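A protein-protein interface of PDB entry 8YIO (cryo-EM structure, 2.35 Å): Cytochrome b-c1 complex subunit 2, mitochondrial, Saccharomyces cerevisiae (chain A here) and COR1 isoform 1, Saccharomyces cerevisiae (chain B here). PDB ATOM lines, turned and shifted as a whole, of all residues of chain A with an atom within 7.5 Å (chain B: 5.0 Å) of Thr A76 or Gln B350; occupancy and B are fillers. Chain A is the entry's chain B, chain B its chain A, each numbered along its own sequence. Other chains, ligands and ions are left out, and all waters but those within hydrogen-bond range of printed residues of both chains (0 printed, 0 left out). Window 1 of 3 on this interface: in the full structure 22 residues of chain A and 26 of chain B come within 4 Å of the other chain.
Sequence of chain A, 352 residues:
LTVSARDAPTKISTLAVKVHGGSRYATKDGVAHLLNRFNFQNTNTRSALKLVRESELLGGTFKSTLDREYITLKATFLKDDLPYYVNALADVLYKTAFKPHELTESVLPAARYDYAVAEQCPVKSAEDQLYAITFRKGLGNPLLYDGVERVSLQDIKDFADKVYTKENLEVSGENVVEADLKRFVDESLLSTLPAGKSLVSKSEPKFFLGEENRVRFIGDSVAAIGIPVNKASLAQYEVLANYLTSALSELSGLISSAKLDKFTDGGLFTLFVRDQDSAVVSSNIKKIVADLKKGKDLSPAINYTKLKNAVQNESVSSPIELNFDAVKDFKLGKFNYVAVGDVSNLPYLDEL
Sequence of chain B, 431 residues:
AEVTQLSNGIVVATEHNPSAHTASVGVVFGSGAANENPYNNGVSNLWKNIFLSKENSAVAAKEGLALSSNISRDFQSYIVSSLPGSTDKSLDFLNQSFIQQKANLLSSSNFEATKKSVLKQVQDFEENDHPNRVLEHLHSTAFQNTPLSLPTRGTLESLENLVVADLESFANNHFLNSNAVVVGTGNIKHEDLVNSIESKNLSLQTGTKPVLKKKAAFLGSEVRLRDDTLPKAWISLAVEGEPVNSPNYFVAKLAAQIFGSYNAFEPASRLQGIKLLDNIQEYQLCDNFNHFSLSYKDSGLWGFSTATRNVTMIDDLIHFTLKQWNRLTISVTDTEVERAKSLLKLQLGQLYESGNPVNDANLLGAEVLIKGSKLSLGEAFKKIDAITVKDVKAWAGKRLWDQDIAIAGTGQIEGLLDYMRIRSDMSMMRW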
ATOM      1  N   ILE A  12     -17.701 -22.688  -5.063  1.00  0.00           N
ATOM      2  CA  ILE A  12     -16.536 -23.507  -5.385  1.00  0.00           C
ATOM      3  C   ILE A  12     -16.963 -24.967  -5.492  1.00  0.00           C
ATOM      4  O   ILE A  12     -17.751 -25.451  -4.675  1.00  0.00           O
ATOM      5  CB  ILE A  12     -15.423 -23.330  -4.324  1.00  0.00           C
ATOM      6  CG1 ILE A  12     -15.135 -21.849  -4.076  1.00  0.00           C
ATOM      7  CG2 ILE A  12     -14.143 -24.041  -4.731  1.00  0.00           C
ATOM      8  CD1 ILE A  12     -14.464 -21.141  -5.225  1.00  0.00           C
ATOM      9  N   SER A  13     -16.444 -25.665  -6.502  1.00  0.00           N
ATOM     10  CA  SER A  13     -16.707 -27.081  -6.718  1.00  0.00           C
ATOM     11  C   SER A  13     -15.412 -27.882  -6.648  1.00  0.00           C
ATOM     12  O   SER A  13     -14.317 -27.347  -6.828  1.00  0.00           O
ATOM     13  CB  SER A  13     -17.388 -27.322  -8.072  1.00  0.00           C
ATOM     14  OG  SER A  13     -18.642 -26.678  -8.136  1.00  0.00           O
ATOM     15  N   THR A  14     -15.552 -29.184  -6.395  1.00  0.00           N
ATOM     16  CA  THR A  14     -14.424 -30.102  -6.316  1.00  0.00           C
ATOM     17  C   THR A  14     -14.780 -31.393  -7.045  1.00  0.00           C
ATOM     18  O   THR A  14     -15.871 -31.935  -6.855  1.00  0.00           O
ATOM     19  CB  THR A  14     -14.046 -30.383  -4.843  1.00  0.00           C
ATOM     20  OG1 THR A  14     -13.553 -29.184  -4.232  1.00  0.00           O
ATOM     21  CG2 THR A  14     -12.970 -31.449  -4.730  1.00  0.00           C
ATOM     22  N   LEU A  15     -13.866 -31.874  -7.889  1.00  0.00           N
ATOM     23  CA  LEU A  15     -14.042 -33.112  -8.640  1.00  0.00           C
ATOM     24  C   LEU A  15     -12.877 -34.053  -8.363  1.00  0.00           C
ATOM     25  O   LEU A  15     -11.720 -33.629  -8.373  1.00  0.00           O
ATOM     26  CB  LEU A  15     -14.140 -32.823 -10.142  1.00  0.00           C
ATOM     27  CG  LEU A  15     -14.614 -33.945 -11.062  1.00  0.00           C
ATOM     28  CD1 LEU A  15     -16.043 -34.338 -10.737  1.00  0.00           C
ATOM     29  CD2 LEU A  15     -14.489 -33.515 -12.508  1.00  0.00           C
ATOM     30  N   SER A  55      -5.791 -22.985 -16.999  1.00  0.00           N
ATOM     31  CA  SER A  55      -6.675 -23.137 -15.854  1.00  0.00           C
ATOM     32  C   SER A  55      -6.504 -22.027 -14.827  1.00  0.00           C
ATOM     33  O   SER A  55      -7.405 -21.822 -14.011  1.00  0.00           O
ATOM     34  CB  SER A  55      -6.457 -24.503 -15.197  1.00  0.00           C
ATOM     35  OG  SER A  55      -5.117 -24.671 -14.785  1.00  0.00           O
ATOM     36  N   GLY A  59      -9.475 -19.938 -13.107  1.00  0.00           N
ATOM     37  CA  GLY A  59      -9.543 -20.074 -11.664  1.00  0.00           C
ATOM     38  C   GLY A  59      -9.644 -21.502 -11.158  1.00  0.00           C
ATOM     39  O   GLY A  59     -10.596 -21.841 -10.453  1.00  0.00           O
ATOM     40  N   GLY A  60      -8.672 -22.344 -11.502  1.00  0.00           N
ATOM     41  CA  GLY A  60      -8.665 -23.720 -11.038  1.00  0.00           C
ATOM     42  C   GLY A  60      -7.258 -24.256 -10.876  1.00  0.00           C
ATOM     43  O   GLY A  60      -6.305 -23.741 -11.465  1.00  0.00           O
ATOM     44  N   THR A  61      -7.138 -25.306 -10.059  1.00  0.00           N
ATOM     45  CA  THR A  61      -5.861 -25.960  -9.792  1.00  0.00           C
ATOM     46  C   THR A  61      -6.046 -27.474  -9.769  1.00  0.00           C
ATOM     47  O   THR A  61      -7.157 -27.980  -9.614  1.00  0.00           O
ATOM     48  CB  THR A  61      -5.233 -25.494  -8.462  1.00  0.00           C
ATOM     49  OG1 THR A  61      -6.234 -25.442  -7.439  1.00  0.00           O
ATOM     50  CG2 THR A  61      -4.578 -24.127  -8.601  1.00  0.00           C
ATOM     51  N   PHE A  62      -4.932 -28.194  -9.918  1.00  0.00           N
ATOM     52  CA  PHE A  62      -4.908 -29.652  -9.959  1.00  0.00           C
ATOM     53  C   PHE A  62      -3.949 -30.201  -8.907  1.00  0.00           C
ATOM     54  O   PHE A  62      -2.979 -29.540  -8.531  1.00  0.00           O
ATOM     55  CB  PHE A  62      -4.474 -30.165 -11.339  1.00  0.00           C
ATOM     56  CG  PHE A  62      -5.440 -29.859 -12.443  1.00  0.00           C
ATOM     57  CD1 PHE A  62      -6.554 -30.657 -12.650  1.00  0.00           C
ATOM     58  CD2 PHE A  62      -5.221 -28.789 -13.295  1.00  0.00           C
ATOM     59  CE1 PHE A  62      -7.437 -30.382 -13.676  1.00  0.00           C
ATOM     60  CE2 PHE A  62      -6.103 -28.509 -14.321  1.00  0.00           C
ATOM     61  CZ  PHE A  62      -7.210 -29.306 -14.512  1.00  0.00           C
ATOM     62  N   LYS A  63      -4.211 -31.429  -8.455  1.00  0.00           N
ATOM     63  CA  LYS A  63      -3.363 -32.086  -7.464  1.00  0.00           C
ATOM     64  C   LYS A  63      -3.536 -33.599  -7.549  1.00  0.00           C
ATOM     65  O   LYS A  63      -4.620 -34.094  -7.860  1.00  0.00           O
ATOM     66  CB  LYS A  63      -3.683 -31.602  -6.045  1.00  0.00           C
ATOM     67  CG  LYS A  63      -2.537 -31.759  -5.068  1.00  0.00           C
ATOM     68  CD  LYS A  63      -2.903 -31.258  -3.687  1.00  0.00           C
ATOM     69  CE  LYS A  63      -1.678 -31.185  -2.793  1.00  0.00           C
ATOM     70  NZ  LYS A  63      -1.101 -32.530  -2.515  1.00  0.00           N
ATOM     71  N   LYS A  74      -7.425 -34.731  -8.351  1.00  0.00           N
ATOM     72  CA  LYS A  74      -8.393 -33.773  -7.833  1.00  0.00           C
ATOM     73  C   LYS A  74      -8.287 -32.438  -8.552  1.00  0.00           C
ATOM     74  O   LYS A  74      -7.196 -32.019  -8.946  1.00  0.00           O
ATOM     75  CB  LYS A  74      -8.200 -33.563  -6.326  1.00  0.00           C
ATOM     76  CG  LYS A  74      -9.448 -33.117  -5.595  1.00  0.00           C
ATOM     77  CD  LYS A  74      -9.168 -32.851  -4.131  1.00  0.00           C
ATOM     78  CE  LYS A  74      -8.187 -31.705  -3.955  1.00  0.00           C
ATOM     79  NZ  LYS A  74      -8.087 -31.255  -2.541  1.00  0.00           N
ATOM     80  N   ALA A  75      -9.427 -31.769  -8.710  1.00  0.00           N
ATOM     81  CA  ALA A  75      -9.495 -30.412  -9.232  1.00  0.00           C
ATOM     82  C   ALA A  75     -10.423 -29.574  -8.361  1.00  0.00           C
ATOM     83  O   ALA A  75     -11.442 -30.069  -7.876  1.00  0.00           O
ATOM     84  CB  ALA A  75      -9.981 -30.395 -10.687  1.00  0.00           C
ATOM     85  N   THR A  76     -10.061 -28.306  -8.167  1.00  0.00           N
ATOM     86  CA  THR A  76     -10.838 -27.344  -7.390  1.00  0.00           C
ATOM     87  C   THR A  76     -10.986 -26.073  -8.212  1.00  0.00           C
ATOM     88  O   THR A  76      -9.984 -25.511  -8.657  1.00  0.00           O
ATOM     89  CB  THR A  76     -10.156 -27.027  -6.051  1.00  0.00           C
ATOM     90  OG1 THR A  76      -9.818 -28.244  -5.377  1.00  0.00           O
ATOM     91  CG2 THR A  76     -11.066 -26.199  -5.164  1.00  0.00           C
ATOM     92  N   PHE A  77     -12.218 -25.605  -8.400  1.00  0.00           N
ATOM     93  CA  PHE A  77     -12.472 -24.628  -9.453  1.00  0.00           C
ATOM     94  C   PHE A  77     -13.762 -23.866  -9.173  1.00  0.00           C
ATOM     95  O   PHE A  77     -14.542 -24.224  -8.292  1.00  0.00           O
ATOM     96  CB  PHE A  77     -12.523 -25.308 -10.832  1.00  0.00           C
ATOM     97  CG  PHE A  77     -13.476 -26.481 -10.914  1.00  0.00           C
ATOM     98  CD1 PHE A  77     -13.062 -27.765 -10.587  1.00  0.00           C
ATOM     99  CD2 PHE A  77     -14.779 -26.301 -11.347  1.00  0.00           C
ATOM    100  CE1 PHE A  77     -13.935 -28.829 -10.660  1.00  0.00           C
ATOM    101  CE2 PHE A  77     -15.656 -27.363 -11.427  1.00  0.00           C
ATOM    102  CZ  PHE A  77     -15.232 -28.629 -11.084  1.00  0.00           C
ATOM    103  N   LEU A  78     -13.972 -22.801  -9.948  1.00  0.00           N
ATOM    104  CA  LEU A  78     -15.228 -22.059  -9.922  1.00  0.00           C
ATOM    105  C   LEU A  78     -16.316 -22.842 -10.649  1.00  0.00           C
ATOM    106  O   LEU A  78     -16.057 -23.461 -11.682  1.00  0.00           O
ATOM    107  CB  LEU A  78     -15.060 -20.683 -10.565  1.00  0.00           C
ATOM    108  CG  LEU A  78     -13.951 -19.769 -10.045  1.00  0.00           C
ATOM    109  CD1 LEU A  78     -13.877 -18.497 -10.866  1.00  0.00           C
ATOM    110  CD2 LEU A  78     -14.153 -19.441  -8.581  1.00  0.00           C
ATOM    111  N   TYR A  85     -12.983 -29.301 -16.833  1.00  0.00           N
ATOM    112  CA  TYR A  85     -12.206 -30.102 -15.898  1.00  0.00           C
ATOM    113  C   TYR A  85     -12.538 -31.584 -15.957  1.00  0.00           C
ATOM    114  O   TYR A  85     -11.720 -32.399 -15.523  1.00  0.00           O
ATOM    115  CB  TYR A  85     -12.395 -29.580 -14.468  1.00  0.00           C
ATOM    116  CG  TYR A  85     -11.837 -28.191 -14.288  1.00  0.00           C
ATOM    117  CD1 TYR A  85     -10.501 -27.992 -13.982  1.00  0.00           C
ATOM    118  CD2 TYR A  85     -12.641 -27.077 -14.463  1.00  0.00           C
ATOM    119  CE1 TYR A  85      -9.988 -26.719 -13.841  1.00  0.00           C
ATOM    120  CE2 TYR A  85     -12.141 -25.808 -14.334  1.00  0.00           C
ATOM    121  CZ  TYR A  85     -10.817 -25.632 -14.017  1.00  0.00           C
ATOM    122  OH  TYR A  85     -10.321 -24.361 -13.878  1.00  0.00           O
ATOM    123  N   LEU B 346     -10.773 -17.612  -6.341  1.00  0.00           N
ATOM    124  CA  LEU B 346     -10.619 -18.992  -5.896  1.00  0.00           C
ATOM    125  C   LEU B 346     -10.078 -19.057  -4.471  1.00  0.00           C
ATOM    126  O   LEU B 346     -10.484 -19.921  -3.688  1.00  0.00           O
ATOM    127  CB  LEU B 346      -9.702 -19.747  -6.862  1.00  0.00           C
ATOM    128  CG  LEU B 346      -9.366 -21.210  -6.563  1.00  0.00           C
ATOM    129  CD1 LEU B 346     -10.596 -22.095  -6.674  1.00  0.00           C
ATOM    130  CD2 LEU B 346      -8.263 -21.703  -7.480  1.00  0.00           C
ATOM    131  N   GLN B 347      -9.178 -18.138  -4.115  1.00  0.00           N
ATOM    132  CA  GLN B 347      -8.593 -18.129  -2.778  1.00  0.00           C
ATOM    133  C   GLN B 347      -9.596 -17.663  -1.727  1.00  0.00           C
ATOM    134  O   GLN B 347      -9.650 -18.223  -0.627  1.00  0.00           O
ATOM    135  CB  GLN B 347      -7.348 -17.242  -2.766  1.00  0.00           C
ATOM    136  CG  GLN B 347      -6.486 -17.400  -1.534  1.00  0.00           C
ATOM    137  CD  GLN B 347      -6.558 -16.200  -0.610  1.00  0.00           C
ATOM    138  OE1 GLN B 347      -6.300 -15.068  -1.017  1.00  0.00           O
ATOM    139  NE2 GLN B 347      -6.933 -16.442   0.639  1.00  0.00           N
ATOM    140  N   LEU B 348     -10.392 -16.639  -2.045  1.00  0.00           N
ATOM    141  CA  LEU B 348     -11.412 -16.163  -1.111  1.00  0.00           C
ATOM    142  C   LEU B 348     -12.538 -17.172  -0.953  1.00  0.00           C
ATOM    143  O   LEU B 348     -13.104 -17.310   0.137  1.00  0.00           O
ATOM    144  CB  LEU B 348     -11.965 -14.819  -1.580  1.00  0.00           C
ATOM    145  CG  LEU B 348     -11.503 -13.567  -0.841  1.00  0.00           C
ATOM    146  CD1 LEU B 348      -9.997 -13.477  -0.813  1.00  0.00           C
ATOM    147  CD2 LEU B 348     -12.094 -12.333  -1.495  1.00  0.00           C
ATOM    148  N   GLY B 349     -12.881 -17.881  -2.029  1.00  0.00           N
ATOM    149  CA  GLY B 349     -13.923 -18.885  -1.947  1.00  0.00           C
ATOM    150  C   GLY B 349     -13.522 -20.106  -1.147  1.00  0.00           C
ATOM    151  O   GLY B 349     -14.379 -20.782  -0.578  1.00  0.00           O
ATOM    152  N   GLN B 350     -12.228 -20.412  -1.093  1.00  0.00           N
ATOM    153  CA  GLN B 350     -11.773 -21.536  -0.285  1.00  0.00           C
ATOM    154  C   GLN B 350     -11.662 -21.170   1.188  1.00  0.00           C
ATOM    155  O   GLN B 350     -11.784 -22.046   2.050  1.00  0.00           O
ATOM    156  CB  GLN B 350     -10.436 -22.088  -0.780  1.00  0.00           C
ATOM    157  CG  GLN B 350     -10.555 -23.040  -1.950  1.00  0.00           C
ATOM    158  CD  GLN B 350      -9.207 -23.450  -2.503  1.00  0.00           C
ATOM    159  OE1 GLN B 350      -8.782 -24.590  -2.348  1.00  0.00           O
ATOM    160  NE2 GLN B 350      -8.531 -22.518  -3.155  1.00  0.00           N
ATOM    161  N   LEU B 351     -11.434 -19.892   1.491  1.00  0.00           N
ATOM    162  CA  LEU B 351     -11.328 -19.459   2.880  1.00  0.00           C
ATOM    163  C   LEU B 351     -12.690 -19.426   3.562  1.00  0.00           C
ATOM    164  O   LEU B 351     -12.814 -19.821   4.726  1.00  0.00           O
ATOM    165  CB  LEU B 351     -10.662 -18.085   2.941  1.00  0.00           C
ATOM    166  CG  LEU B 351     -10.417 -17.458   4.314  1.00  0.00           C
ATOM    167  CD1 LEU B 351      -9.155 -18.016   4.944  1.00  0.00           C
ATOM    168  CD2 LEU B 351     -10.340 -15.946   4.208  1.00  0.00           C
ATOM    169  N   TYR B 352     -13.724 -18.973   2.857  1.00  0.00           N
ATOM    170  CA  TYR B 352     -15.034 -18.789   3.465  1.00  0.00           C
ATOM    171  C   TYR B 352     -15.971 -19.974   3.279  1.00  0.00           C
ATOM    172  O   TYR B 352     -17.032 -20.000   3.905  1.00  0.00           O
ATOM    173  CB  TYR B 352     -15.707 -17.532   2.909  1.00  0.00           C
ATOM    174  CG  TYR B 352     -15.113 -16.250   3.431  1.00  0.00           C
ATOM    175  CD1 TYR B 352     -15.443 -15.774   4.692  1.00  0.00           C
ATOM    176  CD2 TYR B 352     -14.213 -15.520   2.667  1.00  0.00           C
ATOM    177  CE1 TYR B 352     -14.901 -14.605   5.178  1.00  0.00           C
ATOM    178  CE2 TYR B 352     -13.664 -14.351   3.143  1.00  0.00           C
ATOM    179  CZ  TYR B 352     -14.013 -13.897   4.399  1.00  0.00           C
ATOM    180  OH  TYR B 352     -13.469 -12.731   4.882  1.00  0.00           O
ATOM    181  N   GLU B 353     -15.625 -20.946   2.441  1.00  0.00           N
ATOM    182  CA  GLU B 353     -16.509 -22.077   2.176  1.00  0.00           C
ATOM    183  C   GLU B 353     -15.798 -23.396   2.434  1.00  0.00           C
ATOM    184  O   GLU B 353     -15.985 -24.376   1.709  1.00  0.00           O
ATOM    185  CB  GLU B 353     -17.061 -22.033   0.751  1.00  0.00           C
ATOM    186  CG  GLU B 353     -17.691 -20.703   0.364  1.00  0.00           C
ATOM    187  CD  GLU B 353     -18.279 -20.702  -1.027  1.00  0.00           C
ATOM    188  OE1 GLU B 353     -19.474 -20.371  -1.168  1.00  0.00           O
ATOM    189  OE2 GLU B 353     -17.555 -21.036  -1.983  1.00  0.00           O
ATOM    190  N   SER B 354     -14.964 -23.442   3.467  1.00  0.00           N
ATOM    191  CA  SER B 354     -14.474 -24.720   3.949  1.00  0.00           C
ATOM    192  C   SER B 354     -15.560 -25.404   4.777  1.00  0.00           C
ATOM    193  O   SER B 354     -16.568 -24.801   5.153  1.00  0.00           O
ATOM    194  CB  SER B 354     -13.195 -24.541   4.766  1.00  0.00           C
ATOM    195  OG  SER B 354     -13.420 -23.763   5.926  1.00  0.00           O
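N of Ile A12 sits close to OE2 of Glu B353 (3.5 Å).
The backbone carbonyl oxygen (O) of Thr A76 sits at hydrogen-bond distance from the backbone NH (N) of Thr A61 (3.2 Å).
The side-chain amide nitrogen (NE2) of Gln B350 is in hydrogen-bond range of the backbone carbonyl oxygen (O) of Leu B346, at 3.3 Å.
Among the printed residues, merely in contact across the chains: Ile A12 with Gly B349 (3.7 Å), Gly A59 with Leu B346 (3.8 Å), Thr A76 with Leu B346 (3.997 Å) and Thr A76 with Gln B350 (3.97 Å).
Of the printed residues of chain B, Thr A76 touches Leu B346 and Gln B350.
Printed residues of chain A within 4 Å of Leu B346: Gly A59 and Thr A76.
Of the printed residues of chain B, Ile A12 touches Gly B349 and Glu B353.
The nearest printed residue of chain B that does not touch Gly A59 is Gln B347 (7.5 Å).
Along chain B the printed residues that touch a printed residue of chain A span positions 346 to 353.
Of the 16 printed residues of chain A, 3 touch a printed residue of chain B.
Hydrophobic or aromatic side chains of chain A within 4 Å of the printed part of chain B: Ile A12.
Along chain A the printed residues that touch a printed residue of chain B span positions 12 to 76.
Among the printed residues, 5 pairs touch across the chains.
Among the printed residues, no Asp or Glu carboxylate lies within 4 Å of a Lys or Arg side-chain nitrogen of the other chain.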
